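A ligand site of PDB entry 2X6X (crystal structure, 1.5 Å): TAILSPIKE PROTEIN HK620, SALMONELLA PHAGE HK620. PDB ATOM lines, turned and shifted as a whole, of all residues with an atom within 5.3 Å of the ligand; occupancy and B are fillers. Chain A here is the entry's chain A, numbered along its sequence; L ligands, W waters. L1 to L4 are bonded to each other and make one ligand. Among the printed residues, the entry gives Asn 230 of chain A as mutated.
Water W6 bridges O2 of LG4 L4 (2.7 Å) and O of Gly 204 (2.8 Å). Water W9 bridges an oxygen (O1) of LIG L1 (2.7 Å) and the backbone carbonyl oxygen (O) of Gly 102 (2.8 Å). Water W11 lies within hydrogen-bond range of the side-chain hydroxyl of Thr 202 and an oxygen (O4) of LG4 L4. Water W1 bridges an oxygen (O4) of LIG L1 (2.9 Å) and the indole nitrogen (NE1) of Trp 205 (3.1 Å). Water W4 lies within hydrogen-bond range of O2 of LIG L1 and NE2 of Gln 133. Water W3 lies within hydrogen-bond range of ND2 of Asn 230, O of Thr 198 and O6 of LG3 L3.
The backbone NH of Asn 206 sits close to the side-chain amide nitrogen of Asn 237, at 3.1 Å. O of His 103 lies within hydrogen-bond range of NE2 of Gln 133. The side-chain carboxylate (OE2) of Glu 291 is in hydrogen-bond range of the side-chain hydroxyl (OH) of Tyr 235 (2.5 Å).
Residues that only touch the ligand: Trp 199 (3.3 Å), Thr 198 (3.3 Å), Gly 102 (3.6 Å), Trp 205 (3.6 Å), Leu 173 (3.7 Å), Ala 290 (3.7 Å), Thr 202 (3.7 Å) and Phe 138 (3.8 Å). Of the 20 residues printed, 15 come within 4 Å of the ligand. The nearest printed residue that does not touch the ligand is His 288 (4.03 Å).
The side-chain amide oxygen (OD1) of Asn 206 sits at hydrogen-bond distance from an oxygen (O1) of LG4 L4 (2.7 Å). ND1 of His 103 sits at hydrogen-bond distance from O3 of LIG L1. An oxygen (O2) of LG4 L4 lies within hydrogen-bond range of the side-chain amide nitrogen (ND2) of Asn 237 (2.9 Å). OE2 of Glu 291 is in hydrogen-bond range of N1 of LG4 L4, at 2.9 Å. An oxygen (O3) of LIG L1 lies within hydrogen-bond range of the side-chain amide nitrogen of Gln 133 (3.0 Å). OH of Tyr 235 is in hydrogen-bond range of O2 of LG3 L3 (3.1 Å). The side-chain amide nitrogen (ND2) of Asn 230 lies within hydrogen-bond range of an oxygen (O6) of LG3 L3, at 3.4 Å.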
ATOM      1  N   GLY A 102      29.891   4.588   8.323  1.00  0.00           N
ATOM      2  CA  GLY A 102      28.940   4.100   9.323  1.00  0.00           C
ATOM      3  C   GLY A 102      29.205   2.669   9.791  1.00  0.00           C
ATOM      4  O   GLY A 102      28.603   2.221  10.784  1.00  0.00           O
ATOM      5  N   HIS A 103      30.104   1.975   9.107  1.00  0.00           N
ATOM      6  CA  HIS A 103      30.471   0.607   9.438  1.00  0.00           C
ATOM      7  C   HIS A 103      31.910   0.546   9.942  1.00  0.00           C
ATOM      8  O   HIS A 103      32.495  -0.536  10.000  1.00  0.00           O
ATOM      9  CB  HIS A 103      30.324  -0.303   8.202  1.00  0.00           C
ATOM     10  CG  HIS A 103      28.970  -0.250   7.569  1.00  0.00           C
ATOM     11  ND1 HIS A 103      27.928  -1.061   7.963  1.00  0.00           N
ATOM     12  CD2 HIS A 103      28.487   0.505   6.556  1.00  0.00           C
ATOM     13  CE1 HIS A 103      26.865  -0.805   7.215  1.00  0.00           C
ATOM     14  NE2 HIS A 103      27.174   0.147   6.363  1.00  0.00           N
ATOM     15  N   GLN A 133      36.049  -2.315  10.304  1.00  0.00           N
ATOM     16  CA  GLN A 133      35.667  -3.405   9.414  1.00  0.00           C
ATOM     17  C   GLN A 133      36.492  -3.229   8.174  1.00  0.00           C
ATOM     18  O   GLN A 133      36.342  -2.238   7.463  1.00  0.00           O
ATOM     19  CB  GLN A 133      34.167  -3.380   9.102  1.00  0.00           C
ATOM     20  CG  GLN A 133      33.332  -3.589  10.367  1.00  0.00           C
ATOM     21  CD  GLN A 133      31.879  -3.948  10.071  1.00  0.00           C
ATOM     22  OE1 GLN A 133      31.572  -4.916   9.347  1.00  0.00           O
ATOM     23  NE2 GLN A 133      30.954  -3.164  10.651  1.00  0.00           N
ATOM     24  N   PHE A 138      28.832  -2.884   1.777  1.00  0.00           N
ATOM     25  CA  PHE A 138      27.725  -1.930   1.820  1.00  0.00           C
ATOM     26  C   PHE A 138      28.191  -0.626   1.176  1.00  0.00           C
ATOM     27  O   PHE A 138      29.372  -0.299   1.234  1.00  0.00           O
ATOM     28  CB  PHE A 138      27.334  -1.619   3.264  1.00  0.00           C
ATOM     29  CG  PHE A 138      26.777  -2.793   4.046  1.00  0.00           C
ATOM     30  CD1 PHE A 138      25.485  -3.248   3.815  1.00  0.00           C
ATOM     31  CD2 PHE A 138      27.517  -3.382   5.071  1.00  0.00           C
ATOM     32  CE1 PHE A 138      24.958  -4.297   4.573  1.00  0.00           C
ATOM     33  CE2 PHE A 138      26.990  -4.397   5.814  1.00  0.00           C
ATOM     34  CZ  PHE A 138      25.702  -4.854   5.566  1.00  0.00           C
ATOM     35  N   PRO A 143      22.403  -0.085   6.344  1.00  0.00           N
ATOM     36  CA  PRO A 143      22.331  -1.234   5.437  1.00  0.00           C
ATOM     37  C   PRO A 143      20.998  -1.370   4.692  1.00  0.00           C
ATOM     38  O   PRO A 143      20.981  -1.868   3.562  1.00  0.00           O
ATOM     39  CB  PRO A 143      22.596  -2.427   6.357  1.00  0.00           C
ATOM     40  CG  PRO A 143      22.435  -1.966   7.730  1.00  0.00           C
ATOM     41  CD  PRO A 143      22.673  -0.471   7.734  1.00  0.00           C
ATOM     42  N   LEU A 173      32.593  -2.966  17.457  1.00  0.00           N
ATOM     43  CA  LEU A 173      32.525  -4.088  16.530  1.00  0.00           C
ATOM     44  C   LEU A 173      33.757  -4.071  15.638  1.00  0.00           C
ATOM     45  O   LEU A 173      34.226  -2.985  15.238  1.00  0.00           O
ATOM     46  CB  LEU A 173      31.280  -4.011  15.663  1.00  0.00           C
ATOM     47  CG  LEU A 173      29.914  -4.052  16.354  1.00  0.00           C
ATOM     48  CD1 LEU A 173      28.811  -3.723  15.339  1.00  0.00           C
ATOM     49  CD2 LEU A 173      29.648  -5.385  17.036  1.00  0.00           C
ATOM     50  N   THR A 198      35.075  -9.227  16.279  1.00  0.00           N
ATOM     51  CA  THR A 198      33.717  -9.760  16.464  1.00  0.00           C
ATOM     52  C   THR A 198      33.439 -10.904  15.485  1.00  0.00           C
ATOM     53  O   THR A 198      32.876 -11.919  15.856  1.00  0.00           O
ATOM     54  CB  THR A 198      32.654  -8.677  16.242  1.00  0.00           C
ATOM     55  OG1 THR A 198      32.966  -7.485  16.997  1.00  0.00           O
ATOM     56  CG2 THR A 198      31.282  -9.179  16.652  1.00  0.00           C
ATOM     57  N   TRP A 199      33.829 -10.684  14.229  1.00  0.00           N
ATOM     58  CA  TRP A 199      33.729 -11.673  13.132  1.00  0.00           C
ATOM     59  C   TRP A 199      34.994 -11.511  12.280  1.00  0.00           C
ATOM     60  O   TRP A 199      35.608 -10.423  12.288  1.00  0.00           O
ATOM     61  CB  TRP A 199      32.520 -11.423  12.231  1.00  0.00           C
ATOM     62  CG  TRP A 199      31.228 -11.080  12.934  1.00  0.00           C
ATOM     63  CD1 TRP A 199      30.357 -11.940  13.516  1.00  0.00           C
ATOM     64  CD2 TRP A 199      30.657  -9.772  13.087  1.00  0.00           C
ATOM     65  NE1 TRP A 199      29.280 -11.259  14.024  1.00  0.00           N
ATOM     66  CE2 TRP A 199      29.452  -9.922  13.790  1.00  0.00           C
ATOM     67  CE3 TRP A 199      31.079  -8.489  12.727  1.00  0.00           C
ATOM     68  CZ2 TRP A 199      28.643  -8.839  14.121  1.00  0.00           C
ATOM     69  CZ3 TRP A 199      30.287  -7.406  13.055  1.00  0.00           C
ATOM     70  CH2 TRP A 199      29.068  -7.586  13.747  1.00  0.00           C
ATOM     71  N   THR A 202      31.540 -11.697   7.371  1.00  0.00           N
ATOM     72  CA  THR A 202      30.091 -11.782   7.387  1.00  0.00           C
ATOM     73  C   THR A 202      29.593 -11.839   5.926  1.00  0.00           C
ATOM     74  O   THR A 202      30.150 -11.160   5.035  1.00  0.00           O
ATOM     75  CB  THR A 202      29.423 -10.635   8.178  1.00  0.00           C
ATOM     76  OG1 THR A 202      29.664  -9.374   7.552  1.00  0.00           O
ATOM     77  CG2 THR A 202      29.952 -10.596   9.611  1.00  0.00           C
ATOM     78  N   GLY A 204      26.117 -11.574   3.520  1.00  0.00           N
ATOM     79  CA  GLY A 204      24.727 -11.119   3.480  1.00  0.00           C
ATOM     80  C   GLY A 204      24.354 -10.120   4.557  1.00  0.00           C
ATOM     81  O   GLY A 204      25.155  -9.775   5.425  1.00  0.00           O
ATOM     82  N   TRP A 205      23.103  -9.690   4.515  1.00  0.00           N
ATOM     83  CA  TRP A 205      22.560  -8.789   5.510  1.00  0.00           C
ATOM     84  C   TRP A 205      21.066  -9.074   5.649  1.00  0.00           C
ATOM     85  O   TRP A 205      20.317  -8.852   4.715  1.00  0.00           O
ATOM     86  CB  TRP A 205      22.774  -7.302   5.145  1.00  0.00           C
ATOM     87  CG  TRP A 205      22.089  -6.440   6.135  1.00  0.00           C
ATOM     88  CD1 TRP A 205      22.470  -6.219   7.432  1.00  0.00           C
ATOM     89  CD2 TRP A 205      20.850  -5.753   5.968  1.00  0.00           C
ATOM     90  NE1 TRP A 205      21.568  -5.417   8.057  1.00  0.00           N
ATOM     91  CE2 TRP A 205      20.556  -5.118   7.191  1.00  0.00           C
ATOM     92  CE3 TRP A 205      19.973  -5.612   4.900  1.00  0.00           C
ATOM     93  CZ2 TRP A 205      19.416  -4.342   7.359  1.00  0.00           C
ATOM     94  CZ3 TRP A 205      18.828  -4.843   5.073  1.00  0.00           C
ATOM     95  CH2 TRP A 205      18.568  -4.210   6.292  1.00  0.00           C
ATOM     96  N   ASN A 206      20.671  -9.624   6.801  1.00  0.00           N
ATOM     97  CA  ASN A 206      19.262  -9.899   7.132  1.00  0.00           C
ATOM     98  C   ASN A 206      18.519 -10.585   6.009  1.00  0.00           C
ATOM     99  O   ASN A 206      17.420 -10.220   5.634  1.00  0.00           O
ATOM    100  CB  ASN A 206      18.569  -8.614   7.598  1.00  0.00           C
ATOM    101  CG  ASN A 206      19.118  -8.123   8.924  1.00  0.00           C
ATOM    102  OD1 ASN A 206      20.032  -8.735   9.485  1.00  0.00           O
ATOM    103  ND2 ASN A 206      18.584  -7.017   9.410  1.00  0.00           N
ATOM    104  N   ASN A 230      31.860 -10.829  22.296  1.00  0.00           N
ATOM    105  CA  ASN A 230      31.330 -11.978  21.558  1.00  0.00           C
ATOM    106  C   ASN A 230      32.085 -12.134  20.259  1.00  0.00           C
ATOM    107  O   ASN A 230      32.535 -11.144  19.668  1.00  0.00           O
ATOM    108  CB  ASN A 230      29.841 -11.752  21.274  1.00  0.00           C
ATOM    109  CG  ASN A 230      29.182 -12.950  20.589  1.00  0.00           C
ATOM    110  OD1 ASN A 230      29.446 -14.096  20.914  1.00  0.00           O
ATOM    111  ND2 ASN A 230      28.305 -12.656  19.629  1.00  0.00           N
ATOM    112  N   TYR A 235      29.778 -15.401   9.854  1.00  0.00           N
ATOM    113  CA  TYR A 235      28.348 -15.201  10.099  1.00  0.00           C
ATOM    114  C   TYR A 235      27.642 -15.228   8.743  1.00  0.00           C
ATOM    115  O   TYR A 235      27.867 -14.345   7.891  1.00  0.00           O
ATOM    116  CB  TYR A 235      28.108 -13.872  10.815  1.00  0.00           C
ATOM    117  CG  TYR A 235      26.780 -13.679  11.507  1.00  0.00           C
ATOM    118  CD1 TYR A 235      25.621 -13.412  10.789  1.00  0.00           C
ATOM    119  CD2 TYR A 235      26.686 -13.708  12.900  1.00  0.00           C
ATOM    120  CE1 TYR A 235      24.410 -13.205  11.430  1.00  0.00           C
ATOM    121  CE2 TYR A 235      25.481 -13.487  13.546  1.00  0.00           C
ATOM    122  CZ  TYR A 235      24.344 -13.235  12.811  1.00  0.00           C
ATOM    123  OH  TYR A 235      23.141 -13.006  13.469  1.00  0.00           O
ATOM    124  N   ASN A 237      24.509 -14.760   6.739  1.00  0.00           N
ATOM    125  CA  ASN A 237      23.219 -14.079   6.847  1.00  0.00           C
ATOM    126  C   ASN A 237      22.532 -13.866   5.481  1.00  0.00           C
ATOM    127  O   ASN A 237      21.757 -12.944   5.283  1.00  0.00           O
ATOM    128  CB  ASN A 237      23.362 -12.755   7.609  1.00  0.00           C
ATOM    129  CG  ASN A 237      22.105 -12.373   8.358  1.00  0.00           C
ATOM    130  OD1 ASN A 237      21.135 -13.115   8.386  1.00  0.00           O
ATOM    131  ND2 ASN A 237      22.123 -11.208   8.989  1.00  0.00           N
ATOM    132  N   GLU A 263      28.067 -19.039  12.300  1.00  0.00           N
ATOM    133  CA  GLU A 263      26.626 -18.960  12.537  1.00  0.00           C
ATOM    134  C   GLU A 263      25.913 -19.079  11.195  1.00  0.00           C
ATOM    135  O   GLU A 263      26.273 -18.404  10.211  1.00  0.00           O
ATOM    136  CB  GLU A 263      26.191 -17.692  13.244  1.00  0.00           C
ATOM    137  CG  GLU A 263      26.976 -17.400  14.495  1.00  0.00           C
ATOM    138  CD  GLU A 263      26.255 -16.435  15.442  1.00  0.00           C
ATOM    139  OE1 GLU A 263      24.999 -16.402  15.477  1.00  0.00           O
ATOM    140  OE2 GLU A 263      26.957 -15.708  16.182  1.00  0.00           O
ATOM    141  N   HIS A 288      16.580 -15.846  13.541  1.00  0.00           N
ATOM    142  CA  HIS A 288      16.256 -14.615  14.259  1.00  0.00           C
ATOM    143  C   HIS A 288      15.186 -13.881  13.465  1.00  0.00           C
ATOM    144  O   HIS A 288      15.440 -13.480  12.344  1.00  0.00           O
ATOM    145  CB  HIS A 288      17.472 -13.689  14.346  1.00  0.00           C
ATOM    146  CG  HIS A 288      18.517 -14.097  15.338  1.00  0.00           C
ATOM    147  ND1 HIS A 288      18.230 -14.501  16.625  1.00  0.00           N
ATOM    148  CD2 HIS A 288      19.867 -14.088  15.243  1.00  0.00           C
ATOM    149  CE1 HIS A 288      19.356 -14.747  17.262  1.00  0.00           C
ATOM    150  NE2 HIS A 288      20.366 -14.512  16.445  1.00  0.00           N
ATOM    151  N   ALA A 290      14.398 -10.857  13.797  1.00  0.00           N
ATOM    152  CA  ALA A 290      14.972  -9.564  13.435  1.00  0.00           C
ATOM    153  C   ALA A 290      15.777  -9.587  12.122  1.00  0.00           C
ATOM    154  O   ALA A 290      16.107  -8.519  11.578  1.00  0.00           O
ATOM    155  CB  ALA A 290      15.840  -9.014  14.577  1.00  0.00           C
ATOM    156  N   GLU A 291      16.097 -10.789  11.620  1.00  0.00           N
ATOM    157  CA  GLU A 291      16.859 -10.959  10.384  1.00  0.00           C
ATOM    158  C   GLU A 291      16.049 -11.523   9.191  1.00  0.00           C
ATOM    159  O   GLU A 291      16.620 -11.914   8.185  1.00  0.00           O
ATOM    160  CB  GLU A 291      18.088 -11.834  10.670  1.00  0.00           C
ATOM    161  CG  GLU A 291      19.021 -11.253  11.711  1.00  0.00           C
ATOM    162  CD  GLU A 291      20.185 -12.175  12.004  1.00  0.00           C
ATOM    163  OE1 GLU A 291      20.036 -13.404  11.832  1.00  0.00           O
ATOM    164  OE2 GLU A 291      21.232 -11.681  12.425  1.00  0.00           O
ATOM    165  N   ASN A 362      18.080 -14.388  23.011  1.00  0.00           N
ATOM    166  CA  ASN A 362      19.093 -13.481  23.577  1.00  0.00           C
ATOM    167  C   ASN A 362      18.684 -12.867  24.919  1.00  0.00           C
ATOM    168  O   ASN A 362      19.538 -12.589  25.759  1.00  0.00           O
ATOM    169  CB  ASN A 362      19.468 -12.359  22.585  1.00  0.00           C
ATOM    170  CG  ASN A 362      20.255 -12.877  21.368  1.00  0.00           C
ATOM    171  OD1 ASN A 362      20.740 -14.011  21.373  1.00  0.00           O
ATOM    172  ND2 ASN A 362      20.378 -12.037  20.343  1.00  0.00           N
HETATM  173  C1  LIG L   1      25.148  -3.289  12.872  1.00  0.00           C
HETATM  174  C2  LIG L   1      26.138  -2.125  12.941  1.00  0.00           C
HETATM  175  C3  LIG L   1      27.340  -2.332  12.012  1.00  0.00           C
HETATM  176  C4  LIG L   1      26.872  -2.759  10.622  1.00  0.00           C
HETATM  177  C5  LIG L   1      25.928  -3.979  10.718  1.00  0.00           C
HETATM  178  C6  LIG L   1      25.339  -4.364   9.367  1.00  0.00           C
HETATM  179  O1  LIG L   1      25.437  -0.981  12.563  1.00  0.00           O
HETATM  180  O2  LIG L   1      28.124  -1.146  11.900  1.00  0.00           O
HETATM  181  O3  LIG L   1      28.026  -3.027   9.850  1.00  0.00           O
HETATM  182  O4  LIG L   1      24.817  -3.657  11.542  1.00  0.00           O
HETATM  183  C1  LG2 L   2      26.087  -6.699  16.999  1.00  0.00           C
HETATM  184  C2  LG2 L   2      25.611  -5.553  17.888  1.00  0.00           C
HETATM  185  C3  LG2 L   2      24.240  -5.055  17.436  1.00  0.00           C
HETATM  186  C4  LG2 L   2      24.303  -4.679  15.963  1.00  0.00           C
HETATM  187  C5  LG2 L   2      24.821  -5.874  15.149  1.00  0.00           C
HETATM  188  C6  LG2 L   2      25.060  -5.588  13.673  1.00  0.00           C
HETATM  189  O1  LG2 L   2      25.536  -6.074  19.194  1.00  0.00           O
HETATM  190  O2  LG2 L   2      23.819  -3.944  18.210  1.00  0.00           O
HETATM  191  O3  LG2 L   2      23.023  -4.315  15.535  1.00  0.00           O
HETATM  192  O4  LG2 L   2      26.073  -6.272  15.658  1.00  0.00           O
HETATM  193  O5  LG2 L   2      25.701  -4.402  13.528  1.00  0.00           O
HETATM  194  C1  LG3 L   3      24.067 -10.926  17.965  1.00  0.00           C
HETATM  195  C2  LG3 L   3      23.449 -10.312  16.721  1.00  0.00           C
HETATM  196  C3  LG3 L   3      24.606  -9.755  15.880  1.00  0.00           C
HETATM  197  C4  LG3 L   3      25.680  -9.034  16.730  1.00  0.00           C
HETATM  198  C5  LG3 L   3      26.248  -9.960  17.828  1.00  0.00           C
HETATM  199  C6  LG3 L   3      27.176  -9.290  18.840  1.00  0.00           C
HETATM  200  O1  LG3 L   3      24.604 -12.087  17.360  1.00  0.00           O
HETATM  201  O2  LG3 L   3      22.708 -11.262  16.008  1.00  0.00           O
HETATM  202  O3  LG3 L   3      24.045  -8.940  14.878  1.00  0.00           O
HETATM  203  O4  LG3 L   3      25.265  -7.836  17.168  1.00  0.00           O
HETATM  204  O5  LG3 L   3      25.268 -10.625  18.626  1.00  0.00           O
HETATM  205  O6  LG3 L   3      28.507  -9.505  18.496  1.00  0.00           O
HETATM  206  C1  LG4 L   4      23.992  -9.393  13.616  1.00  0.00           C
HETATM  207  C2  LG4 L   4      22.917  -8.605  12.862  1.00  0.00           C
HETATM  208  C3  LG4 L   4      22.919  -8.794  11.340  1.00  0.00           C
HETATM  209  C4  LG4 L   4      24.331  -8.840  10.777  1.00  0.00           C
HETATM  210  C5  LG4 L   4      25.236  -9.684  11.646  1.00  0.00           C
HETATM  211  C6  LG4 L   4      26.662  -9.764  11.113  1.00  0.00           C
HETATM  212  C7  LG4 L   4      20.869  -8.127  14.097  1.00  0.00           C
HETATM  213  C8  LG4 L   4      19.530  -8.627  14.545  1.00  0.00           C
HETATM  214  N1  LG4 L   4      21.601  -8.964  13.372  1.00  0.00           N
HETATM  215  O1  LG4 L   4      22.165  -7.757  10.723  1.00  0.00           O
HETATM  216  O2  LG4 L   4      24.258  -9.375   9.471  1.00  0.00           O
HETATM  217  O3  LG4 L   4      25.253  -9.222  12.995  1.00  0.00           O
HETATM  218  O4  LG4 L   4      27.259  -8.490  11.121  1.00  0.00           O
HETATM  219  O5  LG4 L   4      21.251  -6.996  14.405  1.00  0.00           O
HETATM  220  O   HOH W   1      22.271  -4.857  11.030  1.00  0.00           O
HETATM  221  O   HOH W   2      27.308  -4.200  20.362  1.00  0.00           O
HETATM  222  O   HOH W   3      30.128 -12.112  17.477  1.00  0.00           O
HETATM  223  O   HOH W   4      30.773  -0.733  13.151  1.00  0.00           O
HETATM  224  O   HOH W   5      30.039  -8.098  20.051  1.00  0.00           O
HETATM  225  O   HOH W   6      25.416  -7.948   7.537  1.00  0.00           O
HETATM  226  O   HOH W   7      29.009  -5.150   8.544  1.00  0.00           O
HETATM  227  O   HOH W   8      17.862  -7.870  17.369  1.00  0.00           O
HETATM  228  O   HOH W   9      26.057   0.947  10.816  1.00  0.00           O
HETATM  229  O   HOH W  10      23.539 -14.658  17.000  1.00  0.00           O
HETATM  230  O   HOH W  11      28.030  -7.577   8.647  1.00  0.00           O
